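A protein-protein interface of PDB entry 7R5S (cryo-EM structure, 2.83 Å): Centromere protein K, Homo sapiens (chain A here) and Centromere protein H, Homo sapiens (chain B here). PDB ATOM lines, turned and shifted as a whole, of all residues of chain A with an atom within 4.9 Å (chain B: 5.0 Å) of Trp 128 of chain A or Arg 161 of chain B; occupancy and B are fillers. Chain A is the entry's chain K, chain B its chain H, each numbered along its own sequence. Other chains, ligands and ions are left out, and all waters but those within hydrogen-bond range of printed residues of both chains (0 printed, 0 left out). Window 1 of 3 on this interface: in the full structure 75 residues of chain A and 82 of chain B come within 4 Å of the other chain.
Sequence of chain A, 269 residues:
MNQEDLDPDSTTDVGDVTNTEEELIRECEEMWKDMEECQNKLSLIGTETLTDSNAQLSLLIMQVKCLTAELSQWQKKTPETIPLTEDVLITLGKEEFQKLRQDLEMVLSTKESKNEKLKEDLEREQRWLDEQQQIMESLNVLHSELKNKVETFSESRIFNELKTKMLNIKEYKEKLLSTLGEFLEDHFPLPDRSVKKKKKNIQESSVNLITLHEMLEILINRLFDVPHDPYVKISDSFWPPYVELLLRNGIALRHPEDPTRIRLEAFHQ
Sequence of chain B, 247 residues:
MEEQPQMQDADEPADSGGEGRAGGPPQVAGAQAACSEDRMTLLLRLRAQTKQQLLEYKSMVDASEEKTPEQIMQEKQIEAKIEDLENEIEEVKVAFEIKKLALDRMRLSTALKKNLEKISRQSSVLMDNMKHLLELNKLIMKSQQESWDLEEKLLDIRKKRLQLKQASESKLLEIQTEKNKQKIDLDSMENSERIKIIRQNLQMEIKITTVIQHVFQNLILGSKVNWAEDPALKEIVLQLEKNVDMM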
ATOM      1  N   ARG A 124      25.543   5.600  30.309  1.00  0.00           N
ATOM      2  CA  ARG A 124      25.134   4.196  30.345  1.00  0.00           C
ATOM      3  C   ARG A 124      25.646   3.435  29.125  1.00  0.00           C
ATOM      4  O   ARG A 124      26.126   2.298  29.246  1.00  0.00           O
ATOM      5  CB  ARG A 124      23.613   4.093  30.444  1.00  0.00           C
ATOM      6  CG  ARG A 124      23.126   2.770  31.010  1.00  0.00           C
ATOM      7  CD  ARG A 124      21.607   2.692  31.051  1.00  0.00           C
ATOM      8  NE  ARG A 124      21.014   3.751  31.863  1.00  0.00           N
ATOM      9  CZ  ARG A 124      20.362   4.795  31.365  1.00  0.00           C
ATOM     10  NH1 ARG A 124      20.216   4.926  30.054  1.00  0.00           N
ATOM     11  NH2 ARG A 124      19.854   5.711  32.180  1.00  0.00           N
ATOM     12  N   GLU A 125      25.557   4.048  27.941  1.00  0.00           N
ATOM     13  CA  GLU A 125      26.023   3.392  26.726  1.00  0.00           C
ATOM     14  C   GLU A 125      27.530   3.177  26.756  1.00  0.00           C
ATOM     15  O   GLU A 125      28.022   2.153  26.269  1.00  0.00           O
ATOM     16  CB  GLU A 125      25.623   4.212  25.498  1.00  0.00           C
ATOM     17  CG  GLU A 125      24.132   4.211  25.201  1.00  0.00           C
ATOM     18  CD  GLU A 125      23.666   2.931  24.541  1.00  0.00           C
ATOM     19  OE1 GLU A 125      24.520   2.178  24.028  1.00  0.00           O
ATOM     20  OE2 GLU A 125      22.443   2.675  24.534  1.00  0.00           O
ATOM     21  N   GLN A 126      28.280   4.126  27.320  1.00  0.00           N
ATOM     22  CA  GLN A 126      29.725   3.944  27.442  1.00  0.00           C
ATOM     23  C   GLN A 126      30.052   2.735  28.312  1.00  0.00           C
ATOM     24  O   GLN A 126      30.902   1.903  27.958  1.00  0.00           O
ATOM     25  CB  GLN A 126      30.368   5.209  28.009  1.00  0.00           C
ATOM     26  CG  GLN A 126      31.882   5.143  28.106  1.00  0.00           C
ATOM     27  CD  GLN A 126      32.552   5.134  26.746  1.00  0.00           C
ATOM     28  OE1 GLN A 126      32.262   5.973  25.895  1.00  0.00           O
ATOM     29  NE2 GLN A 126      33.451   4.180  26.536  1.00  0.00           N
ATOM     30  N   ARG A 127      29.383   2.624  29.465  1.00  0.00           N
ATOM     31  CA  ARG A 127      29.630   1.472  30.334  1.00  0.00           C
ATOM     32  C   ARG A 127      29.281   0.160  29.632  1.00  0.00           C
ATOM     33  O   ARG A 127      30.043  -0.819  29.699  1.00  0.00           O
ATOM     34  CB  ARG A 127      28.838   1.613  31.634  1.00  0.00           C
ATOM     35  CG  ARG A 127      29.022   0.449  32.593  1.00  0.00           C
ATOM     36  CD  ARG A 127      28.463   0.771  33.969  1.00  0.00           C
ATOM     37  NE  ARG A 127      27.069   1.198  33.907  1.00  0.00           N
ATOM     38  CZ  ARG A 127      26.031   0.369  33.961  1.00  0.00           C
ATOM     39  NH1 ARG A 127      26.228  -0.936  34.077  1.00  0.00           N
ATOM     40  NH2 ARG A 127      24.795   0.845  33.897  1.00  0.00           N
ATOM     41  N   TRP A 128      28.129   0.125  28.952  1.00  0.00           N
ATOM     42  CA  TRP A 128      27.729  -1.084  28.238  1.00  0.00           C
ATOM     43  C   TRP A 128      28.735  -1.446  27.152  1.00  0.00           C
ATOM     44  O   TRP A 128      29.043  -2.627  26.951  1.00  0.00           O
ATOM     45  CB  TRP A 128      26.337  -0.901  27.636  1.00  0.00           C
ATOM     46  CG  TRP A 128      25.226  -1.112  28.613  1.00  0.00           C
ATOM     47  CD1 TRP A 128      25.294  -1.783  29.799  1.00  0.00           C
ATOM     48  CD2 TRP A 128      23.878  -0.648  28.492  1.00  0.00           C
ATOM     49  NE1 TRP A 128      24.071  -1.765  30.424  1.00  0.00           N
ATOM     50  CE2 TRP A 128      23.184  -1.074  29.641  1.00  0.00           C
ATOM     51  CE3 TRP A 128      23.189   0.088  27.524  1.00  0.00           C
ATOM     52  CZ2 TRP A 128      21.836  -0.790  29.847  1.00  0.00           C
ATOM     53  CZ3 TRP A 128      21.853   0.369  27.730  1.00  0.00           C
ATOM     54  CH2 TRP A 128      21.190  -0.069  28.881  1.00  0.00           C
ATOM     55  N   LEU A 129      29.252  -0.443  26.437  1.00  0.00           N
ATOM     56  CA  LEU A 129      30.238  -0.702  25.393  1.00  0.00           C
ATOM     57  C   LEU A 129      31.513  -1.295  25.974  1.00  0.00           C
ATOM     58  O   LEU A 129      32.093  -2.223  25.397  1.00  0.00           O
ATOM     59  CB  LEU A 129      30.546   0.586  24.631  1.00  0.00           C
ATOM     60  CG  LEU A 129      31.723   0.533  23.654  1.00  0.00           C
ATOM     61  CD1 LEU A 129      31.458  -0.470  22.543  1.00  0.00           C
ATOM     62  CD2 LEU A 129      32.007   1.911  23.079  1.00  0.00           C
ATOM     63  N   ASP A 130      31.972  -0.765  27.110  1.00  0.00           N
ATOM     64  CA  ASP A 130      33.158  -1.330  27.753  1.00  0.00           C
ATOM     65  C   ASP A 130      32.942  -2.796  28.115  1.00  0.00           C
ATOM     66  O   ASP A 130      33.787  -3.660  27.824  1.00  0.00           O
ATOM     67  CB  ASP A 130      33.520  -0.514  28.995  1.00  0.00           C
ATOM     68  CG  ASP A 130      34.426   0.658  28.678  1.00  0.00           C
ATOM     69  OD1 ASP A 130      34.460   1.619  29.475  1.00  0.00           O
ATOM     70  OD2 ASP A 130      35.106   0.620  27.630  1.00  0.00           O
ATOM     71  N   GLU A 131      31.804  -3.098  28.750  1.00  0.00           N
ATOM     72  CA  GLU A 131      31.539  -4.478  29.150  1.00  0.00           C
ATOM     73  C   GLU A 131      31.438  -5.402  27.939  1.00  0.00           C
ATOM     74  O   GLU A 131      31.932  -6.538  27.968  1.00  0.00           O
ATOM     75  CB  GLU A 131      30.265  -4.546  29.990  1.00  0.00           C
ATOM     76  CG  GLU A 131      30.384  -3.849  31.337  1.00  0.00           C
ATOM     77  CD  GLU A 131      29.137  -3.995  32.184  1.00  0.00           C
ATOM     78  OE1 GLU A 131      28.156  -4.599  31.703  1.00  0.00           O
ATOM     79  OE2 GLU A 131      29.136  -3.504  33.332  1.00  0.00           O
ATOM     80  N   GLN A 132      30.815  -4.927  26.857  1.00  0.00           N
ATOM     81  CA  GLN A 132      30.670  -5.759  25.667  1.00  0.00           C
ATOM     82  C   GLN A 132      32.014  -5.994  24.988  1.00  0.00           C
ATOM     83  O   GLN A 132      32.265  -7.084  24.462  1.00  0.00           O
ATOM     84  CB  GLN A 132      29.678  -5.117  24.699  1.00  0.00           C
ATOM     85  CG  GLN A 132      29.005  -6.102  23.763  1.00  0.00           C
ATOM     86  CD  GLN A 132      27.672  -5.599  23.254  1.00  0.00           C
ATOM     87  OE1 GLN A 132      27.223  -4.514  23.623  1.00  0.00           O
ATOM     88  NE2 GLN A 132      27.028  -6.386  22.402  1.00  0.00           N
ATOM     89  N   ASP B 156      28.071   7.010  17.295  1.00  0.00           N
ATOM     90  CA  ASP B 156      29.220   6.126  17.128  1.00  0.00           C
ATOM     91  C   ASP B 156      29.280   5.074  18.228  1.00  0.00           C
ATOM     92  O   ASP B 156      29.642   3.917  17.966  1.00  0.00           O
ATOM     93  CB  ASP B 156      30.515   6.939  17.095  1.00  0.00           C
ATOM     94  CG  ASP B 156      30.490   8.031  16.045  1.00  0.00           C
ATOM     95  OD1 ASP B 156      30.716   7.721  14.857  1.00  0.00           O
ATOM     96  OD2 ASP B 156      30.250   9.202  16.407  1.00  0.00           O
ATOM     97  N   ILE B 157      28.935   5.451  19.464  1.00  0.00           N
ATOM     98  CA  ILE B 157      28.947   4.462  20.545  1.00  0.00           C
ATOM     99  C   ILE B 157      27.998   3.308  20.222  1.00  0.00           C
ATOM    100  O   ILE B 157      28.364   2.126  20.317  1.00  0.00           O
ATOM    101  CB  ILE B 157      28.601   5.124  21.890  1.00  0.00           C
ATOM    102  CG1 ILE B 157      29.781   5.964  22.382  1.00  0.00           C
ATOM    103  CG2 ILE B 157      28.230   4.071  22.921  1.00  0.00           C
ATOM    104  CD1 ILE B 157      29.646   6.430  23.812  1.00  0.00           C
ATOM    105  N   ARG B 158      26.768   3.638  19.818  1.00  0.00           N
ATOM    106  CA  ARG B 158      25.786   2.600  19.516  1.00  0.00           C
ATOM    107  C   ARG B 158      26.201   1.770  18.306  1.00  0.00           C
ATOM    108  O   ARG B 158      25.959   0.556  18.267  1.00  0.00           O
ATOM    109  CB  ARG B 158      24.412   3.232  19.298  1.00  0.00           C
ATOM    110  CG  ARG B 158      23.805   3.807  20.566  1.00  0.00           C
ATOM    111  CD  ARG B 158      22.635   4.727  20.268  1.00  0.00           C
ATOM    112  NE  ARG B 158      22.017   5.222  21.494  1.00  0.00           N
ATOM    113  CZ  ARG B 158      21.105   6.188  21.535  1.00  0.00           C
ATOM    114  NH1 ARG B 158      20.702   6.769  20.414  1.00  0.00           N
ATOM    115  NH2 ARG B 158      20.596   6.573  22.697  1.00  0.00           N
ATOM    116  N   LYS B 159      26.830   2.402  17.311  1.00  0.00           N
ATOM    117  CA  LYS B 159      27.288   1.655  16.142  1.00  0.00           C
ATOM    118  C   LYS B 159      28.337   0.616  16.529  1.00  0.00           C
ATOM    119  O   LYS B 159      28.277  -0.544  16.089  1.00  0.00           O
ATOM    120  CB  LYS B 159      27.841   2.622  15.094  1.00  0.00           C
ATOM    121  CG  LYS B 159      28.072   1.998  13.730  1.00  0.00           C
ATOM    122  CD  LYS B 159      28.420   3.058  12.698  1.00  0.00           C
ATOM    123  CE  LYS B 159      27.344   4.129  12.623  1.00  0.00           C
ATOM    124  NZ  LYS B 159      27.687   5.196  11.645  1.00  0.00           N
ATOM    125  N   LYS B 160      29.307   1.015  17.356  1.00  0.00           N
ATOM    126  CA  LYS B 160      30.322   0.065  17.803  1.00  0.00           C
ATOM    127  C   LYS B 160      29.702  -1.066  18.615  1.00  0.00           C
ATOM    128  O   LYS B 160      30.082  -2.238  18.461  1.00  0.00           O
ATOM    129  CB  LYS B 160      31.399   0.786  18.614  1.00  0.00           C
ATOM    130  CG  LYS B 160      32.342   1.628  17.771  1.00  0.00           C
ATOM    131  CD  LYS B 160      33.500   2.165  18.596  1.00  0.00           C
ATOM    132  CE  LYS B 160      33.015   3.118  19.674  1.00  0.00           C
ATOM    133  NZ  LYS B 160      34.146   3.696  20.451  1.00  0.00           N
ATOM    134  N   ARG B 161      28.743  -0.736  19.488  1.00  0.00           N
ATOM    135  CA  ARG B 161      28.060  -1.778  20.253  1.00  0.00           C
ATOM    136  C   ARG B 161      27.369  -2.781  19.335  1.00  0.00           C
ATOM    137  O   ARG B 161      27.447  -3.998  19.555  1.00  0.00           O
ATOM    138  CB  ARG B 161      27.049  -1.150  21.210  1.00  0.00           C
ATOM    139  CG  ARG B 161      27.633  -0.679  22.527  1.00  0.00           C
ATOM    140  CD  ARG B 161      26.525  -0.375  23.515  1.00  0.00           C
ATOM    141  NE  ARG B 161      25.615  -1.507  23.659  1.00  0.00           N
ATOM    142  CZ  ARG B 161      24.353  -1.404  24.063  1.00  0.00           C
ATOM    143  NH1 ARG B 161      23.845  -0.218  24.362  1.00  0.00           N
ATOM    144  NH2 ARG B 161      23.598  -2.489  24.163  1.00  0.00           N
ATOM    145  N   LEU B 162      26.683  -2.286  18.301  1.00  0.00           N
ATOM    146  CA  LEU B 162      25.976  -3.180  17.389  1.00  0.00           C
ATOM    147  C   LEU B 162      26.945  -4.083  16.636  1.00  0.00           C
ATOM    148  O   LEU B 162      26.673  -5.275  16.444  1.00  0.00           O
ATOM    149  CB  LEU B 162      25.124  -2.369  16.412  1.00  0.00           C
ATOM    150  CG  LEU B 162      24.148  -3.165  15.546  1.00  0.00           C
ATOM    151  CD1 LEU B 162      23.333  -4.125  16.397  1.00  0.00           C
ATOM    152  CD2 LEU B 162      23.236  -2.230  14.771  1.00  0.00           C
ATOM    153  N   GLN B 163      28.082  -3.535  16.199  1.00  0.00           N
ATOM    154  CA  GLN B 163      29.078  -4.361  15.518  1.00  0.00           C
ATOM    155  C   GLN B 163      29.595  -5.467  16.434  1.00  0.00           C
ATOM    156  O   GLN B 163      29.723  -6.632  16.022  1.00  0.00           O
ATOM    157  CB  GLN B 163      30.231  -3.492  15.017  1.00  0.00           C
ATOM    158  CG  GLN B 163      29.837  -2.497  13.939  1.00  0.00           C
ATOM    159  CD  GLN B 163      31.037  -1.894  13.239  1.00  0.00           C
ATOM    160  OE1 GLN B 163      31.165  -0.674  13.141  1.00  0.00           O
ATOM    161  NE2 GLN B 163      31.926  -2.749  12.746  1.00  0.00           N
ATOM    162  N   LEU B 164      29.901  -5.117  17.688  1.00  0.00           N
ATOM    163  CA  LEU B 164      30.384  -6.119  18.634  1.00  0.00           C
ATOM    164  C   LEU B 164      29.353  -7.219  18.854  1.00  0.00           C
ATOM    165  O   LEU B 164      29.701  -8.407  18.904  1.00  0.00           O
ATOM    166  CB  LEU B 164      30.747  -5.457  19.962  1.00  0.00           C
ATOM    167  CG  LEU B 164      32.018  -4.612  19.968  1.00  0.00           C
ATOM    168  CD1 LEU B 164      32.134  -3.861  21.278  1.00  0.00           C
ATOM    169  CD2 LEU B 164      33.239  -5.486  19.739  1.00  0.00           C
ATOM    170  N   LYS B 165      28.080  -6.841  18.997  1.00  0.00           N
ATOM    171  CA  LYS B 165      27.026  -7.839  19.170  1.00  0.00           C
ATOM    172  C   LYS B 165      26.940  -8.762  17.959  1.00  0.00           C
ATOM    173  O   LYS B 165      26.832  -9.990  18.101  1.00  0.00           O
ATOM    174  CB  LYS B 165      25.687  -7.144  19.414  1.00  0.00           C
ATOM    175  CG  LYS B 165      24.483  -8.069  19.344  1.00  0.00           C
ATOM    176  CD  LYS B 165      23.185  -7.295  19.487  1.00  0.00           C
ATOM    177  CE  LYS B 165      21.977  -8.210  19.367  1.00  0.00           C
ATOM    178  NZ  LYS B 165      21.937  -8.904  18.051  1.00  0.00           N
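Ile 157 of chain B touches Glu 125 of chain A.
Gln 126 of chain A touches Ile 157 of chain B.
Arg 161 of chain B touches Trp 128 of chain A.
Leu 129 of chain A touches Lys 160 of chain B.
Leu 129 of chain A touches Arg 161 of chain B (CB to CG, 3.8 Å).
Leu 164 of chain B touches Leu 129 of chain A.
Lys 165 of chain B touches Gln 132 of chain A (CB to NE2, 3.4 Å).
NH1 of Arg 161 of chain B is in salt-bridge range of OE1 of Glu 125 of chain A (2.5 Å).
The guanidinium group of Arg 158 of chain B lies within salt-bridge range of the side-chain carboxylate of Glu 125 of chain A (3.99 Å).
NE of Arg 161 of chain B sits at hydrogen-bond distance from OE1 of Gln 132 of chain A (3.4 Å).
Of the printed residues of chain B, Trp 128 of chain A touches Arg 161 (3.2 Å).
Of the printed residues of chain A, Arg 161 of chain B touches Glu 125, Trp 128, Leu 129 and Gln 132.
Of the printed residues of chain A, Ile 157 of chain B touches Glu 125 and Gln 126.
Printed residues of chain A within 4 Å of Lys 160 of chain B: Leu 129.
Printed residues of chain B within 4 Å of Gln 126 of chain A: Ile 157.
Printed residues of chain B within 4 Å of Gln 132 of chain A: Arg 161 and Lys 165.
Gln 163 of chain B touches none of the printed residues of chain A.
The nearest printed residue of chain A that does not touch Arg 161 of chain B is Arg 124 of chain A (5.9 Å).
The nearest printed residue of chain B that does not touch Gln 126 of chain A is Lys 160 of chain B (6.1 Å).
Of the 10 printed residues of chain B, 6 touch a printed residue of chain A.
Printed residues of chain B that touch a printed residue of chain A: Ile 157, Arg 158, Lys 160, Arg 161, Leu 164 and Lys 165.
Hydrophobic or aromatic side chains of chain B that line the printed part of chain A: Ile 157 and Leu 164.
Printed residues of chain A that touch a printed residue of chain B: Glu 125, Gln 126, Trp 128, Leu 129 and Gln 132.
Hydrophobic or aromatic side chains of chain A that line the printed part of chain B: Trp 128 and Leu 129.
Among the printed residues, 10 pairs touch across the chains.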
